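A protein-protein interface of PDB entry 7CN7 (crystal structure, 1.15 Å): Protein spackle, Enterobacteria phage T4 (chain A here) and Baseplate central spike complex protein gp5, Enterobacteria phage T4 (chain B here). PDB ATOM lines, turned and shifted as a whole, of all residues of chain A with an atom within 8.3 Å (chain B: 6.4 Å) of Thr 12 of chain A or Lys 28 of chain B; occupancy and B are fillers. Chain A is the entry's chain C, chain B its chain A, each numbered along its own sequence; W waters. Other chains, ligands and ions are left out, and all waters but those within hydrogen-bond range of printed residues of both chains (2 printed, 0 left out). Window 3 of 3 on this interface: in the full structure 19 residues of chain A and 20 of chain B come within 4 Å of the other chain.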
ATOM      1  N   ASP A   5      -7.700 -18.479   2.040  1.00  0.00           N
ATOM      2  CA  ASP A   5      -8.974 -18.986   1.557  1.00  0.00           C
ATOM      3  C   ASP A   5     -10.057 -17.923   1.620  1.00  0.00           C
ATOM      4  O   ASP A   5     -10.858 -17.802   0.681  1.00  0.00           O
ATOM      5  CB  ASP A   5      -9.383 -20.230   2.337  1.00  0.00           C
ATOM      6  CG  ASP A   5      -8.467 -21.406   2.047  1.00  0.00           C
ATOM      7  OD1 ASP A   5      -8.281 -22.242   2.943  1.00  0.00           O
ATOM      8  OD2 ASP A   5      -7.944 -21.485   0.914  1.00  0.00           O
ATOM      9  N   LEU A   6     -10.122 -17.169   2.726  1.00  0.00           N
ATOM     10  CA  LEU A   6     -11.148 -16.144   2.823  1.00  0.00           C
ATOM     11  C   LEU A   6     -10.864 -14.974   1.886  1.00  0.00           C
ATOM     12  O   LEU A   6     -11.802 -14.321   1.413  1.00  0.00           O
ATOM     13  CB  LEU A   6     -11.316 -15.653   4.259  1.00  0.00           C
ATOM     14  CG  LEU A   6     -12.127 -16.598   5.142  1.00  0.00           C
ATOM     15  CD1 LEU A   6     -11.938 -16.238   6.596  1.00  0.00           C
ATOM     16  CD2 LEU A   6     -13.587 -16.552   4.790  1.00  0.00           C
ATOM     17  N   CYS A   7      -9.597 -14.679   1.613  1.00  0.00           N
ATOM     18  CA  CYS A   7      -9.298 -13.613   0.660  1.00  0.00           C
ATOM     19  C   CYS A   7      -9.855 -13.975  -0.710  1.00  0.00           C
ATOM     20  O   CYS A   7     -10.657 -13.230  -1.287  1.00  0.00           O
ATOM     21  CB  CYS A   7      -7.797 -13.384   0.590  1.00  0.00           C
ATOM     22  SG  CYS A   7      -7.366 -12.090  -0.595  1.00  0.00           S
ATOM     23  N   GLU A   8      -9.480 -15.150  -1.212  1.00  0.00           N
ATOM     24  CA  GLU A   8      -9.932 -15.571  -2.529  1.00  0.00           C
ATOM     25  C   GLU A   8     -11.448 -15.656  -2.593  1.00  0.00           C
ATOM     26  O   GLU A   8     -12.059 -15.196  -3.563  1.00  0.00           O
ATOM     27  CB  GLU A   8      -9.271 -16.910  -2.894  1.00  0.00           C
ATOM     28  CG  GLU A   8      -7.745 -16.885  -2.876  1.00  0.00           C
ATOM     29  CD  GLU A   8      -7.191 -15.863  -3.855  1.00  0.00           C
ATOM     30  OE1 GLU A   8      -7.701 -15.860  -4.982  1.00  0.00           O
ATOM     31  OE2 GLU A   8      -6.304 -15.038  -3.495  1.00  0.00           O
ATOM     32  N   TRP A   9     -12.060 -16.287  -1.596  1.00  0.00           N
ATOM     33  CA  TRP A   9     -13.503 -16.463  -1.583  1.00  0.00           C
ATOM     34  C   TRP A   9     -14.213 -15.121  -1.479  1.00  0.00           C
ATOM     35  O   TRP A   9     -15.180 -14.867  -2.190  1.00  0.00           O
ATOM     36  CB  TRP A   9     -13.861 -17.404  -0.440  1.00  0.00           C
ATOM     37  CG  TRP A   9     -15.303 -17.681  -0.272  1.00  0.00           C
ATOM     38  CD1 TRP A   9     -16.051 -18.653  -0.901  1.00  0.00           C
ATOM     39  CD2 TRP A   9     -16.180 -17.015   0.623  1.00  0.00           C
ATOM     40  NE1 TRP A   9     -17.333 -18.610  -0.447  1.00  0.00           N
ATOM     41  CE2 TRP A   9     -17.441 -17.623   0.493  1.00  0.00           C
ATOM     42  CE3 TRP A   9     -16.022 -15.983   1.543  1.00  0.00           C
ATOM     43  CZ2 TRP A   9     -18.535 -17.233   1.251  1.00  0.00           C
ATOM     44  CZ3 TRP A   9     -17.114 -15.594   2.296  1.00  0.00           C
ATOM     45  CH2 TRP A   9     -18.357 -16.216   2.136  1.00  0.00           C
ATOM     46  N   SER A  10     -13.744 -14.234  -0.608  1.00  0.00           N
ATOM     47  CA  SER A  10     -14.445 -12.963  -0.461  1.00  0.00           C
ATOM     48  C   SER A  10     -14.376 -12.135  -1.737  1.00  0.00           C
ATOM     49  O   SER A  10     -15.290 -11.364  -2.021  1.00  0.00           O
ATOM     50  CB  SER A  10     -13.893 -12.150   0.714  1.00  0.00           C
ATOM     51  OG  SER A  10     -12.622 -11.594   0.444  1.00  0.00           O
ATOM     52  N   MET A  11     -13.295 -12.270  -2.516  1.00  0.00           N
ATOM     53  CA  MET A  11     -13.177 -11.527  -3.754  1.00  0.00           C
ATOM     54  C   MET A  11     -14.107 -12.046  -4.830  1.00  0.00           C
ATOM     55  O   MET A  11     -14.341 -11.330  -5.806  1.00  0.00           O
ATOM     56  CB  MET A  11     -11.733 -11.592  -4.278  1.00  0.00           C
ATOM     57  CG  MET A  11     -10.745 -10.765  -3.466  1.00  0.00           C
ATOM     58  SD  MET A  11      -9.137 -10.586  -4.253  1.00  0.00           S
ATOM     59  CE  MET A  11      -8.549 -12.294  -4.286  1.00  0.00           C
ATOM     60  N   THR A  12     -14.599 -13.275  -4.706  1.00  0.00           N
ATOM     61  CA  THR A  12     -15.218 -13.963  -5.834  1.00  0.00           C
ATOM     62  C   THR A  12     -16.599 -14.546  -5.575  1.00  0.00           C
ATOM     63  O   THR A  12     -17.321 -14.757  -6.548  1.00  0.00           O
ATOM     64  CB  THR A  12     -14.297 -15.081  -6.359  1.00  0.00           C
ATOM     65  OG1 THR A  12     -14.090 -16.043  -5.316  1.00  0.00           O
ATOM     66  CG2 THR A  12     -12.978 -14.549  -6.890  1.00  0.00           C
ATOM     67  N   ALA A  13     -16.973 -14.853  -4.339  1.00  0.00           N
ATOM     68  CA  ALA A  13     -18.225 -15.550  -4.080  1.00  0.00           C
ATOM     69  C   ALA A  13     -19.431 -14.602  -4.164  1.00  0.00           C
ATOM     70  O   ALA A  13     -19.307 -13.385  -4.231  1.00  0.00           O
ATOM     71  CB  ALA A  13     -18.128 -16.263  -2.736  1.00  0.00           C
ATOM     72  N   ASP A  14     -20.611 -15.197  -4.125  1.00  0.00           N
ATOM     73  CA  ASP A  14     -21.863 -14.456  -4.127  1.00  0.00           C
ATOM     74  C   ASP A  14     -21.849 -13.381  -3.064  1.00  0.00           C
ATOM     75  O   ASP A  14     -21.520 -13.640  -1.905  1.00  0.00           O
ATOM     76  CB  ASP A  14     -22.960 -15.494  -3.824  1.00  0.00           C
ATOM     77  CG  ASP A  14     -24.288 -14.905  -3.488  1.00  0.00           C
ATOM     78  OD1 ASP A  14     -25.010 -14.676  -4.458  1.00  0.00           O
ATOM     79  OD2 ASP A  14     -24.632 -14.723  -2.285  1.00  0.00           O
ATOM     80  N   GLN A  15     -22.284 -12.183  -3.443  1.00  0.00           N
ATOM     81  CA  GLN A  15     -22.264 -11.067  -2.507  1.00  0.00           C
ATOM     82  C   GLN A  15     -22.957 -11.398  -1.196  1.00  0.00           C
ATOM     83  O   GLN A  15     -22.463 -11.035  -0.116  1.00  0.00           O
ATOM     84  CB  GLN A  15     -22.907  -9.839  -3.135  1.00  0.00           C
ATOM     85  CG  GLN A  15     -23.096  -8.694  -2.156  1.00  0.00           C
ATOM     86  CD  GLN A  15     -23.468  -7.402  -2.852  1.00  0.00           C
ATOM     87  OE1 GLN A  15     -23.864  -7.386  -4.013  1.00  0.00           O
ATOM     88  NE2 GLN A  15     -23.331  -6.316  -2.155  1.00  0.00           N
ATOM     89  N   VAL A  18     -20.866 -13.570   0.994  1.00  0.00           N
ATOM     90  CA  VAL A  18     -19.666 -12.898   1.467  1.00  0.00           C
ATOM     91  C   VAL A  18     -20.008 -11.907   2.566  1.00  0.00           C
ATOM     92  O   VAL A  18     -19.320 -11.828   3.591  1.00  0.00           O
ATOM     93  CB  VAL A  18     -18.916 -12.235   0.295  1.00  0.00           C
ATOM     94  CG1 VAL A  18     -17.744 -11.399   0.823  1.00  0.00           C
ATOM     95  CG2 VAL A  18     -18.407 -13.309  -0.657  1.00  0.00           C
ATOM     96  N   MET A  51     -19.360  -5.004   2.046  1.00  0.00           N
ATOM     97  CA  MET A  51     -18.398  -5.664   1.171  1.00  0.00           C
ATOM     98  C   MET A  51     -17.024  -5.022   1.219  1.00  0.00           C
ATOM     99  O   MET A  51     -16.019  -5.713   1.028  1.00  0.00           O
ATOM    100  CB  MET A  51     -18.898  -5.657  -0.278  1.00  0.00           C
ATOM    101  CG  MET A  51     -17.905  -6.302  -1.216  1.00  0.00           C
ATOM    102  SD  MET A  51     -17.697  -8.079  -0.904  1.00  0.00           S
ATOM    103  CE  MET A  51     -19.230  -8.638  -1.650  1.00  0.00           C
ATOM    104  N   ASN A  54     -13.688  -6.459   2.921  1.00  0.00           N
ATOM    105  CA  ASN A  54     -13.057  -7.743   2.636  1.00  0.00           C
ATOM    106  C   ASN A  54     -11.544  -7.634   2.577  1.00  0.00           C
ATOM    107  O   ASN A  54     -10.830  -8.537   3.033  1.00  0.00           O
ATOM    108  CB  ASN A  54     -13.607  -8.371   1.351  1.00  0.00           C
ATOM    109  CG  ASN A  54     -13.020  -7.819   0.067  1.00  0.00           C
ATOM    110  OD1 ASN A  54     -12.994  -6.617  -0.180  1.00  0.00           O
ATOM    111  ND2 ASN A  54     -12.553  -8.731  -0.777  1.00  0.00           N
ATOM    112  N   LEU B  25     -11.888  -5.007  -2.510  1.00  0.00           N
ATOM    113  CA  LEU B  25     -11.330  -5.566  -3.738  1.00  0.00           C
ATOM    114  C   LEU B  25     -12.198  -6.743  -4.162  1.00  0.00           C
ATOM    115  O   LEU B  25     -12.208  -7.785  -3.502  1.00  0.00           O
ATOM    116  CB  LEU B  25      -9.873  -5.970  -3.547  1.00  0.00           C
ATOM    117  CG  LEU B  25      -8.999  -6.098  -4.798  1.00  0.00           C
ATOM    118  CD1 LEU B  25      -7.595  -6.574  -4.365  1.00  0.00           C
ATOM    119  CD2 LEU B  25      -9.563  -7.039  -5.822  1.00  0.00           C
ATOM    120  N   ARG B  26     -12.911  -6.580  -5.269  1.00  0.00           N
ATOM    121  CA  ARG B  26     -13.768  -7.621  -5.799  1.00  0.00           C
ATOM    122  C   ARG B  26     -13.334  -8.000  -7.207  1.00  0.00           C
ATOM    123  O   ARG B  26     -13.060  -7.132  -8.035  1.00  0.00           O
ATOM    124  CB  ARG B  26     -15.226  -7.188  -5.802  1.00  0.00           C
ATOM    125  CG  ARG B  26     -15.882  -7.393  -4.431  1.00  0.00           C
ATOM    126  CD  ARG B  26     -16.197  -8.857  -4.178  1.00  0.00           C
ATOM    127  NE  ARG B  26     -17.304  -9.336  -5.025  1.00  0.00           N
ATOM    128  CZ  ARG B  26     -17.912 -10.501  -4.864  1.00  0.00           C
ATOM    129  NH1 ARG B  26     -17.540 -11.317  -3.876  1.00  0.00           N
ATOM    130  NH2 ARG B  26     -18.898 -10.861  -5.688  1.00  0.00           N
ATOM    131  N   LEU B  27     -13.334  -9.306  -7.485  1.00  0.00           N
ATOM    132  CA  LEU B  27     -13.076  -9.820  -8.816  1.00  0.00           C
ATOM    133  C   LEU B  27     -14.339 -10.346  -9.474  1.00  0.00           C
ATOM    134  O   LEU B  27     -14.298 -10.743 -10.635  1.00  0.00           O
ATOM    135  CB  LEU B  27     -11.959 -10.844  -8.799  1.00  0.00           C
ATOM    136  CG  LEU B  27     -10.628 -10.310  -8.270  1.00  0.00           C
ATOM    137  CD1 LEU B  27      -9.608 -11.432  -8.241  1.00  0.00           C
ATOM    138  CD2 LEU B  27     -10.124  -9.131  -9.102  1.00  0.00           C
ATOM    139  N   LYS B  28     -15.465 -10.318  -8.777  1.00  0.00           N
ATOM    140  CA  LYS B  28     -16.765 -10.547  -9.386  1.00  0.00           C
ATOM    141  C   LYS B  28     -17.714  -9.434  -8.968  1.00  0.00           C
ATOM    142  O   LYS B  28     -17.548  -8.785  -7.928  1.00  0.00           O
ATOM    143  CB  LYS B  28     -17.352 -11.921  -9.064  1.00  0.00           C
ATOM    144  CG  LYS B  28     -16.479 -13.079  -9.512  1.00  0.00           C
ATOM    145  CD  LYS B  28     -17.304 -14.335  -9.692  1.00  0.00           C
ATOM    146  CE  LYS B  28     -16.477 -15.586  -9.887  1.00  0.00           C
ATOM    147  NZ  LYS B  28     -17.393 -16.777  -9.971  1.00  0.00           N
ATOM    148  N   VAL B  29     -18.724  -9.216  -9.804  1.00  0.00           N
ATOM    149  CA  VAL B  29     -19.676  -8.135  -9.608  1.00  0.00           C
ATOM    150  C   VAL B  29     -20.327  -8.224  -8.231  1.00  0.00           C
ATOM    151  O   VAL B  29     -20.639  -9.306  -7.715  1.00  0.00           O
ATOM    152  CB  VAL B  29     -20.743  -8.162 -10.720  1.00  0.00           C
ATOM    153  CG1 VAL B  29     -21.822  -7.113 -10.491  1.00  0.00           C
ATOM    154  CG2 VAL B  29     -20.119  -7.987 -12.109  1.00  0.00           C
ATOM    155  N   TYR B  30     -20.561  -7.058  -7.654  1.00  0.00           N
ATOM    156  CA  TYR B  30     -21.403  -6.879  -6.488  1.00  0.00           C
ATOM    157  C   TYR B  30     -22.157  -5.576  -6.682  1.00  0.00           C
ATOM    158  O   TYR B  30     -21.912  -4.828  -7.636  1.00  0.00           O
ATOM    159  CB  TYR B  30     -20.593  -6.873  -5.197  1.00  0.00           C
ATOM    160  CG  TYR B  30     -19.733  -5.663  -4.952  1.00  0.00           C
ATOM    161  CD1 TYR B  30     -18.539  -5.489  -5.632  1.00  0.00           C
ATOM    162  CD2 TYR B  30     -20.085  -4.715  -4.001  1.00  0.00           C
ATOM    163  CE1 TYR B  30     -17.714  -4.388  -5.388  1.00  0.00           C
ATOM    164  CE2 TYR B  30     -19.281  -3.638  -3.739  1.00  0.00           C
ATOM    165  CZ  TYR B  30     -18.086  -3.484  -4.421  1.00  0.00           C
ATOM    166  OH  TYR B  30     -17.314  -2.385  -4.109  1.00  0.00           O
ATOM    167  N   THR B  38     -20.884  -2.935  -9.372  1.00  0.00           N
ATOM    168  CA  THR B  38     -19.534  -2.504  -9.042  1.00  0.00           C
ATOM    169  C   THR B  38     -18.612  -3.714  -9.115  1.00  0.00           C
ATOM    170  O   THR B  38     -19.042  -4.861  -8.923  1.00  0.00           O
ATOM    171  CB  THR B  38     -19.556  -1.888  -7.623  1.00  0.00           C
ATOM    172  OG1 THR B  38     -20.555  -0.864  -7.576  1.00  0.00           O
ATOM    173  CG2 THR B  38     -18.253  -1.281  -7.224  1.00  0.00           C
ATOM    174  N   ILE B  39     -17.324  -3.458  -9.355  1.00  0.00           N
ATOM    175  CA  ILE B  39     -16.325  -4.519  -9.331  1.00  0.00           C
ATOM    176  C   ILE B  39     -14.976  -3.878  -9.042  1.00  0.00           C
ATOM    177  O   ILE B  39     -14.848  -2.650  -8.999  1.00  0.00           O
ATOM    178  CB  ILE B  39     -16.352  -5.313 -10.657  1.00  0.00           C
ATOM    179  CG1 ILE B  39     -15.718  -6.701 -10.562  1.00  0.00           C
ATOM    180  CG2 ILE B  39     -15.772  -4.466 -11.789  1.00  0.00           C
ATOM    181  CD1 ILE B  39     -16.107  -7.622 -11.693  1.00  0.00           C
ATOM    182  N   GLY B  40     -13.950  -4.691  -8.856  1.00  0.00           N
ATOM    183  CA  GLY B  40     -12.620  -4.148  -8.657  1.00  0.00           C
ATOM    184  C   GLY B  40     -12.515  -3.388  -7.356  1.00  0.00           C
ATOM    185  O   GLY B  40     -13.020  -3.820  -6.308  1.00  0.00           O
ATOM    186  N   GLY B  70     -19.786 -15.484 -16.758  1.00  0.00           N
ATOM    187  CA  GLY B  70     -20.208 -15.836 -15.424  1.00  0.00           C
ATOM    188  C   GLY B  70     -21.357 -14.986 -14.918  1.00  0.00           C
ATOM    189  O   GLY B  70     -21.655 -13.910 -15.426  1.00  0.00           O
ATOM    190  N   ASN B  71     -22.005 -15.483 -13.869  1.00  0.00           N
ATOM    191  CA  ASN B  71     -23.029 -14.731 -13.160  1.00  0.00           C
ATOM    192  C   ASN B  71     -22.835 -15.030 -11.687  1.00  0.00           C
ATOM    193  O   ASN B  71     -23.234 -16.103 -11.225  1.00  0.00           O
ATOM    194  CB  ASN B  71     -24.439 -15.094 -13.600  1.00  0.00           C
ATOM    195  CG  ASN B  71     -25.459 -14.241 -12.906  1.00  0.00           C
ATOM    196  OD1 ASN B  71     -25.087 -13.380 -12.114  1.00  0.00           O
ATOM    197  ND2 ASN B  71     -26.721 -14.453 -13.197  1.00  0.00           N
ATOM    198  N   PRO B  72     -22.197 -14.130 -10.928  1.00  0.00           N
ATOM    199  CA  PRO B  72     -21.803 -12.775 -11.313  1.00  0.00           C
ATOM    200  C   PRO B  72     -20.590 -12.760 -12.246  1.00  0.00           C
ATOM    201  O   PRO B  72     -19.735 -13.636 -12.197  1.00  0.00           O
ATOM    202  CB  PRO B  72     -21.496 -12.121  -9.967  1.00  0.00           C
ATOM    203  CG  PRO B  72     -21.044 -13.251  -9.070  1.00  0.00           C
ATOM    204  CD  PRO B  72     -21.895 -14.416  -9.506  1.00  0.00           C
ATOM    205  N   GLY B  73     -20.507 -11.727 -13.078  1.00  0.00           N
ATOM    206  CA  GLY B  73     -19.388 -11.619 -13.998  1.00  0.00           C
ATOM    207  C   GLY B  73     -18.068 -11.458 -13.276  1.00  0.00           C
ATOM    208  O   GLY B  73     -17.989 -10.853 -12.205  1.00  0.00           O
ATOM    209  N   SER B  74     -17.023 -11.978 -13.906  1.00  0.00           N
ATOM    210  CA  SER B  74     -15.689 -12.084 -13.334  1.00  0.00           C
ATOM    211  C   SER B  74     -14.647 -11.320 -14.144  1.00  0.00           C
ATOM    212  O   SER B  74     -14.674 -11.320 -15.380  1.00  0.00           O
ATOM    213  CB  SER B  74     -15.338 -13.580 -13.298  1.00  0.00           C
ATOM    214  OG  SER B  74     -14.010 -13.812 -12.930  1.00  0.00           O
ATOM    215  N   ILE B  75     -13.671 -10.756 -13.432  1.00  0.00           N
ATOM    216  CA  ILE B  75     -12.472 -10.168 -14.013  1.00  0.00           C
ATOM    217  C   ILE B  75     -11.251 -10.749 -13.312  1.00  0.00           C
ATOM    218  O   ILE B  75     -11.353 -11.375 -12.252  1.00  0.00           O
ATOM    219  CB  ILE B  75     -12.475  -8.626 -13.950  1.00  0.00           C
ATOM    220  CG1 ILE B  75     -12.459  -8.122 -12.499  1.00  0.00           C
ATOM    221  CG2 ILE B  75     -13.654  -8.073 -14.736  1.00  0.00           C
ATOM    222  CD1 ILE B  75     -12.307  -6.613 -12.381  1.00  0.00           C
HETATM  223  O   HOH W   1     -18.821 -16.751  -7.526  1.00  0.00           O
HETATM  224  O   HOH W   2     -22.192 -11.257  -6.245  1.00  0.00           O
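Water W1 bridges the backbone carbonyl oxygen of Thr 12 of chain A (2.7 Å) and the side-chain amino group of Lys 28 of chain B (2.8 Å).
Water W2 lies within hydrogen-bond range of the backbone carbonyl oxygen of Val 29 of chain B, the backbone NH of Gln 15 of chain A and the guanidinium group of Arg 26 of chain B.
Printed residues of chain B within 4 Å of Ser 10 of chain A: Arg 26.
Thr 12 of chain A touches just these residues of chain B: Arg 26 and Lys 28.
Of the printed residues of chain B, Ala 13 of chain A touches Arg 26.
Printed residues of chain B within 4 Å of Met 51 of chain A: Arg 26 and Tyr 30.
Printed residues of chain A within 4 Å of Leu 25 of chain B: Met 11 and Asn 54.
Of chain A, only Met 11 (3.3 Å) and Thr 12 (3.2 Å) come within 4 Å of Lys 28 of chain B.
Pro 72 of chain B touches none of the printed residues of chain A.
Gly 73 of chain B touches none of the printed residues of chain A.
O of Leu 25 of chain B sits at hydrogen-bond distance from ND2 of Asn 54 of chain A.
NH1 of Arg 26 of chain B lies within hydrogen-bond range of O of Ser 10 of chain A (2.9 Å).
The guanidinium group (NH1) of Arg 26 of chain B is in hydrogen-bond range of the backbone carbonyl oxygen (O) of Ala 13 of chain A, at 2.7 Å.
The backbone NH (N) of Leu 27 of chain B is in hydrogen-bond range of the backbone carbonyl oxygen (O) of Met 11 of chain A.
The backbone NH of Lys 28 of chain B lies within hydrogen-bond range of the backbone carbonyl oxygen of Met 11 of chain A (3.3 Å).
The backbone carbonyl oxygen of Lys 28 of chain B lies within hydrogen-bond range of the guanidinium group of Arg 26 of chain B (3.0 Å).
O of Arg 26 of chain B is in hydrogen-bond range of N of Gly 40 of chain B.
The backbone NH of Thr 38 of chain B lies within hydrogen-bond range of the backbone carbonyl oxygen of Tyr 30 of chain B (2.8 Å).
O of Cys 7 of chain A sits at hydrogen-bond distance from OG of Ser 10 of chain A (3.1 Å).
OG of Ser 10 of chain A is in hydrogen-bond range of ND2 of Asn 54 of chain A (3.1 Å).
The backbone carbonyl oxygen of Met 51 of chain A lies close to the side-chain amide oxygen of Asn 54 of chain A, at 3.4 Å.
Hydrophobic or aromatic side chains of chain A within 4 Å of the printed part of chain B: Met 11, Val 18 and Met 51.
Hydrophobic or aromatic side chains of chain B that line the printed part of chain A: Leu 25, Leu 27 and Tyr 30.
Among the printed residues, 13 pairs touch across the chains.
Among the printed residues, no Asp or Glu carboxylate lies within 4 Å of a Lys or Arg side-chain nitrogen of the other chain.
Among the printed residues, pairs that only touch across the chains: Thr 12 of chain A with Lys 28 of chain B (3.2 Å), Met 11 of chain A with Leu 25 of chain B (3.3 Å), Met 11 of chain A with Arg 26 of chain B (3.5 Å), Gln 15 of chain A with Tyr 30 of chain B (3.5 Å), Thr 12 of chain A with Arg 26 of chain B (3.6 Å), Met 51 of chain A with Arg 26 of chain B (3.7 Å), Met 51 of chain A with Tyr 30 of chain B (3.9 Å) and Val 18 of chain A with Arg 26 of chain B (3.9 Å).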
